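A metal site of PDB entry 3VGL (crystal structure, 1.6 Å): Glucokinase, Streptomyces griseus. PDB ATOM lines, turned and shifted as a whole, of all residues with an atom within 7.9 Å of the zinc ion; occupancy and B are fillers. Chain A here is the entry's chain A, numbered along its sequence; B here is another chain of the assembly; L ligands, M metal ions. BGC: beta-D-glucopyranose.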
ATOM      1  N   TYR A  67      27.568  14.454  -8.993  1.00  0.00           N
ATOM      2  CA  TYR A  67      27.915  13.757  -7.756  1.00  0.00           C
ATOM      3  C   TYR A  67      29.433  13.769  -7.657  1.00  0.00           C
ATOM      4  O   TYR A  67      30.114  13.161  -8.478  1.00  0.00           O
ATOM      5  CB  TYR A  67      27.435  12.286  -7.862  1.00  0.00           C
ATOM      6  CG  TYR A  67      25.940  12.049  -7.634  1.00  0.00           C
ATOM      7  CD1 TYR A  67      24.974  12.716  -8.399  1.00  0.00           C
ATOM      8  CD2 TYR A  67      25.500  11.127  -6.679  1.00  0.00           C
ATOM      9  CE1 TYR A  67      23.614  12.454  -8.202  1.00  0.00           C
ATOM     10  CE2 TYR A  67      24.119  10.859  -6.485  1.00  0.00           C
ATOM     11  CZ  TYR A  67      23.202  11.572  -7.234  1.00  0.00           C
ATOM     12  OH  TYR A  67      21.837  11.350  -7.047  1.00  0.00           O
ATOM     13  N   PHE A  77      29.298  10.934 -11.082  1.00  0.00           N
ATOM     14  CA  PHE A  77      28.073  10.721 -11.856  1.00  0.00           C
ATOM     15  C   PHE A  77      27.446  12.111 -12.087  1.00  0.00           C
ATOM     16  O   PHE A  77      27.397  12.920 -11.160  1.00  0.00           O
ATOM     17  CB  PHE A  77      27.148   9.808 -11.019  1.00  0.00           C
ATOM     18  CG  PHE A  77      25.835   9.494 -11.649  1.00  0.00           C
ATOM     19  CD1 PHE A  77      25.733   8.474 -12.591  1.00  0.00           C
ATOM     20  CD2 PHE A  77      24.692  10.182 -11.265  1.00  0.00           C
ATOM     21  CE1 PHE A  77      24.495   8.163 -13.167  1.00  0.00           C
ATOM     22  CE2 PHE A  77      23.442   9.869 -11.825  1.00  0.00           C
ATOM     23  CZ  PHE A  77      23.349   8.861 -12.784  1.00  0.00           C
ATOM     24  N   PRO A  79      23.783  13.834 -14.041  1.00  0.00           N
ATOM     25  CA  PRO A  79      22.609  13.539 -14.865  1.00  0.00           C
ATOM     26  C   PRO A  79      22.484  14.351 -16.137  1.00  0.00           C
ATOM     27  O   PRO A  79      21.856  13.885 -17.108  1.00  0.00           O
ATOM     28  CB  PRO A  79      21.413  13.856 -13.922  1.00  0.00           C
ATOM     29  CG  PRO A  79      21.943  14.692 -12.915  1.00  0.00           C
ATOM     30  CD  PRO A  79      23.424  14.405 -12.739  1.00  0.00           C
ATOM     31  N   ASN A  80      23.052  15.559 -16.169  1.00  0.00           N
ATOM     32  CA  ASN A  80      22.821  16.474 -17.279  1.00  0.00           C
ATOM     33  C   ASN A  80      24.118  16.866 -18.018  1.00  0.00           C
ATOM     34  O   ASN A  80      24.100  17.732 -18.873  1.00  0.00           O
ATOM     35  CB  ASN A  80      22.063  17.709 -16.788  1.00  0.00           C
ATOM     36  CG  ASN A  80      20.742  17.348 -16.135  1.00  0.00           C
ATOM     37  OD1 ASN A  80      19.949  16.614 -16.719  1.00  0.00           O
ATOM     38  ND2 ASN A  80      20.515  17.848 -14.923  1.00  0.00           N
ATOM     39  N   GLU A 154      22.017  15.645  -2.714  1.00  0.00           N
ATOM     40  CA  GLU A 154      21.529  15.449  -4.075  1.00  0.00           C
ATOM     41  C   GLU A 154      19.998  15.512  -4.086  1.00  0.00           C
ATOM     42  O   GLU A 154      19.293  14.565  -4.469  1.00  0.00           O
ATOM     43  CB  GLU A 154      22.080  14.140  -4.638  1.00  0.00           C
ATOM     44  CG  GLU A 154      23.520  14.325  -5.147  1.00  0.00           C
ATOM     45  CD  GLU A 154      23.579  15.346  -6.258  1.00  0.00           C
ATOM     46  OE1 GLU A 154      22.663  15.302  -7.121  1.00  0.00           O
ATOM     47  OE2 GLU A 154      24.533  16.169  -6.237  1.00  0.00           O
ATOM     48  N   PHE A 155      19.498  16.673  -3.646  1.00  0.00           N
ATOM     49  CA  PHE A 155      18.062  16.837  -3.450  1.00  0.00           C
ATOM     50  C   PHE A 155      17.263  16.700  -4.751  1.00  0.00           C
ATOM     51  O   PHE A 155      16.061  16.349  -4.740  1.00  0.00           O
ATOM     52  CB  PHE A 155      17.746  18.245  -2.916  1.00  0.00           C
ATOM     53  CG  PHE A 155      18.416  18.606  -1.611  1.00  0.00           C
ATOM     54  CD1 PHE A 155      18.859  17.637  -0.706  1.00  0.00           C
ATOM     55  CD2 PHE A 155      18.518  19.948  -1.274  1.00  0.00           C
ATOM     56  CE1 PHE A 155      19.455  18.024   0.514  1.00  0.00           C
ATOM     57  CE2 PHE A 155      19.099  20.350  -0.075  1.00  0.00           C
ATOM     58  CZ  PHE A 155      19.574  19.390   0.817  1.00  0.00           C
ATOM     59  N   GLY A 156      17.920  16.966  -5.874  1.00  0.00           N
ATOM     60  CA  GLY A 156      17.248  16.928  -7.181  1.00  0.00           C
ATOM     61  C   GLY A 156      16.717  15.564  -7.541  1.00  0.00           C
ATOM     62  O   GLY A 156      15.847  15.451  -8.383  1.00  0.00           O
ATOM     63  N   HIS A 157      17.237  14.521  -6.877  1.00  0.00           N
ATOM     64  CA  HIS A 157      16.844  13.156  -7.213  1.00  0.00           C
ATOM     65  C   HIS A 157      16.078  12.439  -6.124  1.00  0.00           C
ATOM     66  O   HIS A 157      15.895  11.225  -6.154  1.00  0.00           O
ATOM     67  CB  HIS A 157      18.085  12.365  -7.716  1.00  0.00           C
ATOM     68  CG  HIS A 157      18.816  13.127  -8.761  1.00  0.00           C
ATOM     69  ND1 HIS A 157      18.324  13.290 -10.034  1.00  0.00           N
ATOM     70  CD2 HIS A 157      19.919  13.926  -8.650  1.00  0.00           C
ATOM     71  CE1 HIS A 157      19.124  14.113 -10.700  1.00  0.00           C
ATOM     72  NE2 HIS A 157      20.096  14.504  -9.893  1.00  0.00           N
ATOM     73  N   ILE A 158      15.546  13.221  -5.184  1.00  0.00           N
ATOM     74  CA  ILE A 158      14.531  12.703  -4.265  1.00  0.00           C
ATOM     75  C   ILE A 158      13.274  12.468  -5.089  1.00  0.00           C
ATOM     76  O   ILE A 158      12.919  13.288  -5.943  1.00  0.00           O
ATOM     77  CB  ILE A 158      14.204  13.773  -3.173  1.00  0.00           C
ATOM     78  CG1 ILE A 158      15.429  13.961  -2.268  1.00  0.00           C
ATOM     79  CG2 ILE A 158      12.961  13.371  -2.348  1.00  0.00           C
ATOM     80  CD1 ILE A 158      15.328  15.298  -1.507  1.00  0.00           C
ATOM     81  N   ARG A 159      12.590  11.362  -4.864  1.00  0.00           N
ATOM     82  CA  ARG A 159      11.423  11.017  -5.691  1.00  0.00           C
ATOM     83  C   ARG A 159      10.200  11.702  -5.131  1.00  0.00           C
ATOM     84  O   ARG A 159       9.767  11.418  -3.987  1.00  0.00           O
ATOM     85  CB  ARG A 159      11.200   9.503  -5.672  1.00  0.00           C
ATOM     86  CG  ARG A 159      10.051   9.107  -6.568  1.00  0.00           C
ATOM     87  CD  ARG A 159       9.754   7.615  -6.511  1.00  0.00           C
ATOM     88  NE  ARG A 159       9.160   7.219  -5.227  1.00  0.00           N
ATOM     89  CZ  ARG A 159       8.697   6.001  -4.986  1.00  0.00           C
ATOM     90  NH1 ARG A 159       8.205   5.704  -3.776  1.00  0.00           N
ATOM     91  NH2 ARG A 159       8.683   5.099  -5.959  1.00  0.00           N
ATOM     92  N   LEU A 165       8.056  11.604 -13.986  1.00  0.00           N
ATOM     93  CA  LEU A 165       8.830  11.974 -15.172  1.00  0.00           C
ATOM     94  C   LEU A 165      10.216  11.333 -15.228  1.00  0.00           C
ATOM     95  O   LEU A 165      10.893  11.264 -14.206  1.00  0.00           O
ATOM     96  CB  LEU A 165       9.021  13.492 -15.151  1.00  0.00           C
ATOM     97  CG  LEU A 165       7.781  14.297 -15.547  1.00  0.00           C
ATOM     98  CD1 LEU A 165       8.011  15.774 -15.148  1.00  0.00           C
ATOM     99  CD2 LEU A 165       7.476  14.146 -17.067  1.00  0.00           C
ATOM    100  N   LEU A 166      10.654  10.917 -16.413  1.00  0.00           N
ATOM    101  CA  LEU A 166      12.027  10.453 -16.600  1.00  0.00           C
ATOM    102  C   LEU A 166      13.041  11.540 -16.274  1.00  0.00           C
ATOM    103  O   LEU A 166      12.901  12.673 -16.743  1.00  0.00           O
ATOM    104  CB  LEU A 166      12.225   9.974 -18.038  1.00  0.00           C
ATOM    105  CG  LEU A 166      11.405   8.789 -18.525  1.00  0.00           C
ATOM    106  CD1 LEU A 166      11.559   8.710 -20.032  1.00  0.00           C
ATOM    107  CD2 LEU A 166      11.865   7.509 -17.865  1.00  0.00           C
ATOM    108  N   CYS A 167      14.079  11.153 -15.538  1.00  0.00           N
ATOM    109  CA  CYS A 167      15.174  12.057 -15.171  1.00  0.00           C
ATOM    110  C   CYS A 167      16.486  11.633 -15.826  1.00  0.00           C
ATOM    111  O   CYS A 167      16.653  10.465 -16.132  1.00  0.00           O
ATOM    112  CB  CYS A 167      15.351  12.088 -13.635  1.00  0.00           C
ATOM    113  SG  CYS A 167      16.511  13.327 -13.022  1.00  0.00           S
ATOM    114  N   GLY A 168      17.401  12.588 -16.034  1.00  0.00           N
ATOM    115  CA  GLY A 168      18.737  12.314 -16.564  1.00  0.00           C
ATOM    116  C   GLY A 168      19.536  11.342 -15.716  1.00  0.00           C
ATOM    117  O   GLY A 168      20.488  10.706 -16.213  1.00  0.00           O
ATOM    118  N   CYS A 169      19.174  11.201 -14.438  1.00  0.00           N
ATOM    119  CA  CYS A 169      19.854  10.237 -13.574  1.00  0.00           C
ATOM    120  C   CYS A 169      19.487   8.789 -13.856  1.00  0.00           C
ATOM    121  O   CYS A 169      20.133   7.869 -13.343  1.00  0.00           O
ATOM    122  CB  CYS A 169      19.604  10.557 -12.099  1.00  0.00           C
ATOM    123  SG  CYS A 169      17.918  10.145 -11.575  1.00  0.00           S
ATOM    124  N   GLY A 170      18.465   8.591 -14.682  1.00  0.00           N
ATOM    125  CA  GLY A 170      17.989   7.254 -15.024  1.00  0.00           C
ATOM    126  C   GLY A 170      16.784   6.767 -14.246  1.00  0.00           C
ATOM    127  O   GLY A 170      16.217   5.697 -14.550  1.00  0.00           O
ATOM    128  N   SER A 171      16.386   7.561 -13.247  1.00  0.00           N
ATOM    129  CA  SER A 171      15.197   7.225 -12.436  1.00  0.00           C
ATOM    130  C   SER A 171      13.986   8.038 -12.858  1.00  0.00           C
ATOM    131  O   SER A 171      14.074   8.858 -13.782  1.00  0.00           O
ATOM    132  CB  SER A 171      15.493   7.528 -10.971  1.00  0.00           C
ATOM    133  OG  SER A 171      16.447   6.549 -10.496  1.00  0.00           O
ATOM    134  N   GLN A 172      12.865   7.830 -12.176  1.00  0.00           N
ATOM    135  CA  GLN A 172      11.627   8.547 -12.485  1.00  0.00           C
ATOM    136  C   GLN A 172      11.131   9.333 -11.285  1.00  0.00           C
ATOM    137  O   GLN A 172      11.236   8.883 -10.144  1.00  0.00           O
ATOM    138  CB  GLN A 172      10.519   7.547 -12.827  1.00  0.00           C
ATOM    139  CG  GLN A 172      10.604   7.004 -14.243  1.00  0.00           C
ATOM    140  CD  GLN A 172       9.533   5.978 -14.502  1.00  0.00           C
ATOM    141  OE1 GLN A 172       8.320   6.296 -14.582  1.00  0.00           O
ATOM    142  NE2 GLN A 172       9.942   4.724 -14.626  1.00  0.00           N
ATOM    143  N   GLY A 173      10.527  10.476 -11.574  1.00  0.00           N
ATOM    144  CA  GLY A 173       9.794  11.236 -10.546  1.00  0.00           C
ATOM    145  C   GLY A 173      10.636  12.145  -9.677  1.00  0.00           C
ATOM    146  O   GLY A 173      10.149  12.672  -8.682  1.00  0.00           O
ATOM    147  N   CYS A 174      11.899  12.307 -10.044  1.00  0.00           N
ATOM    148  CA  CYS A 174      12.823  13.171  -9.297  1.00  0.00           C
ATOM    149  C   CYS A 174      12.352  14.615  -9.175  1.00  0.00           C
ATOM    150  O   CYS A 174      11.797  15.225 -10.116  1.00  0.00           O
ATOM    151  CB  CYS A 174      14.150  13.155 -10.015  1.00  0.00           C
ATOM    152  SG  CYS A 174      14.934  11.554 -10.088  1.00  0.00           S
ATOM    153  N   TRP A 175      12.602  15.180  -7.988  1.00  0.00           N
ATOM    154  CA  TRP A 175      12.244  16.571  -7.734  1.00  0.00           C
ATOM    155  C   TRP A 175      12.692  17.528  -8.851  1.00  0.00           C
ATOM    156  O   TRP A 175      11.955  18.418  -9.248  1.00  0.00           O
ATOM    157  CB  TRP A 175      12.797  16.996  -6.354  1.00  0.00           C
ATOM    158  CG  TRP A 175      12.269  18.319  -5.846  1.00  0.00           C
ATOM    159  CD1 TRP A 175      11.107  18.972  -6.210  1.00  0.00           C
ATOM    160  CD2 TRP A 175      12.854  19.070  -4.789  1.00  0.00           C
ATOM    161  NE1 TRP A 175      10.978  20.132  -5.471  1.00  0.00           N
ATOM    162  CE2 TRP A 175      12.018  20.203  -4.578  1.00  0.00           C
ATOM    163  CE3 TRP A 175      13.996  18.905  -3.996  1.00  0.00           C
ATOM    164  CZ2 TRP A 175      12.311  21.187  -3.617  1.00  0.00           C
ATOM    165  CZ3 TRP A 175      14.287  19.877  -3.026  1.00  0.00           C
ATOM    166  CH2 TRP A 175      13.447  20.997  -2.856  1.00  0.00           C
ATOM    167  N   GLU A 176      13.887  17.327  -9.382  1.00  0.00           N
ATOM    168  CA  GLU A 176      14.383  18.274 -10.368  1.00  0.00           C
ATOM    169  C   GLU A 176      13.575  18.301 -11.662  1.00  0.00           C
ATOM    170  O   GLU A 176      13.593  19.311 -12.372  1.00  0.00           O
ATOM    171  CB  GLU A 176      15.875  18.081 -10.627  1.00  0.00           C
ATOM    172  CG  GLU A 176      16.262  17.156 -11.691  1.00  0.00           C
ATOM    173  CD  GLU A 176      17.756  17.320 -12.091  1.00  0.00           C
ATOM    174  OE1 GLU A 176      18.551  17.735 -11.233  1.00  0.00           O
ATOM    175  OE2 GLU A 176      18.111  17.027 -13.254  1.00  0.00           O
ATOM    176  N   GLN A 177      12.836  17.234 -11.964  1.00  0.00           N
ATOM    177  CA  GLN A 177      11.955  17.266 -13.147  1.00  0.00           C
ATOM    178  C   GLN A 177      10.736  18.161 -12.960  1.00  0.00           C
ATOM    179  O   GLN A 177      10.103  18.517 -13.944  1.00  0.00           O
ATOM    180  CB  GLN A 177      11.524  15.846 -13.545  1.00  0.00           C
ATOM    181  CG  GLN A 177      12.705  14.959 -13.944  1.00  0.00           C
ATOM    182  CD  GLN A 177      13.493  15.588 -15.056  1.00  0.00           C
ATOM    183  OE1 GLN A 177      12.919  16.128 -16.045  1.00  0.00           O
ATOM    184  NE2 GLN A 177      14.811  15.564 -14.918  1.00  0.00           N
ATOM    185  N   ILE B 282      19.804   5.847  -6.358  1.00  0.00           N
ATOM    186  CA  ILE B 282      20.095   6.627  -7.601  1.00  0.00           C
ATOM    187  C   ILE B 282      21.524   6.331  -8.056  1.00  0.00           C
ATOM    188  O   ILE B 282      22.422   6.253  -7.236  1.00  0.00           O
ATOM    189  CB  ILE B 282      19.994   8.206  -7.358  1.00  0.00           C
ATOM    190  CG1 ILE B 282      18.585   8.673  -6.937  1.00  0.00           C
ATOM    191  CG2 ILE B 282      20.371   8.989  -8.613  1.00  0.00           C
ATOM    192  CD1 ILE B 282      17.478   8.397  -7.958  1.00  0.00           C
ATOM    193  N   GLY B 283      21.728   6.246  -9.368  1.00  0.00           N
ATOM    194  CA  GLY B 283      23.073   6.317  -9.925  1.00  0.00           C
ATOM    195  C   GLY B 283      23.691   4.953 -10.140  1.00  0.00           C
ATOM    196  O   GLY B 283      24.853   4.852 -10.568  1.00  0.00           O
HETATM  197  C2  BGC L   1      22.961  17.162 -10.205  1.00  0.00           C
HETATM  198  C3  BGC L   1      23.569  17.885  -9.012  1.00  0.00           C
HETATM  199  C4  BGC L   1      23.740  19.381  -9.281  1.00  0.00           C
HETATM  200  C5  BGC L   1      22.401  19.922  -9.774  1.00  0.00           C
HETATM  201  C6  BGC L   1      22.466  21.415 -10.106  1.00  0.00           C
HETATM  202  C1  BGC L   1      21.662  17.867 -10.583  1.00  0.00           C
HETATM  203  O1  BGC L   1      21.103  17.307 -11.741  1.00  0.00           O
HETATM  204  O2  BGC L   1      22.644  15.830  -9.781  1.00  0.00           O
HETATM  205  O3  BGC L   1      24.809  17.337  -8.677  1.00  0.00           O
HETATM  206  O4  BGC L   1      24.083  20.048  -8.074  1.00  0.00           O
HETATM  207  O5  BGC L   1      21.946  19.215 -10.918  1.00  0.00           O
HETATM  208  O6  BGC L   1      23.429  21.662 -11.127  1.00  0.00           O
HETATM  209 ZN    ZN M   1      16.916  12.111 -11.083  1.00  0.00          ZN
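A ring nitrogen (NE2) of His 157 is in hydrogen-bond range of an oxygen (O2) of the ligand (2.9 Å). The side-chain carboxylate of Glu 176 is in hydrogen-bond range of an oxygen (O1) of the ligand (2.6 Å). O2 of the ligand lies within hydrogen-bond range of OE1 of Glu 154 (2.7 Å). The side-chain amide nitrogen (ND2) of Asn 80 sits at hydrogen-bond distance from an oxygen (O1) of the ligand, at 3.3 Å.
The side-chain sulfur (SG) of Cys 169 sits close to the backbone NH (N) of Ser 171 (3.4 Å). SG of Cys 167 lies close to NE2 of Gln 177.
Of the 25 residues printed, 4 come within 4 Å of the zinc ion. The nearest printed residue that does not touch the zinc ion is Gly 156 (4.4 Å).
The zinc ion is bound by ND1 of His 157 (2.1 Å), SG of Cys 169 (2.3 Å), SG of Cys 174 (2.3 Å) and SG of Cys 167 (2.3 Å). The zinc ion has four donor atoms within binding distance.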
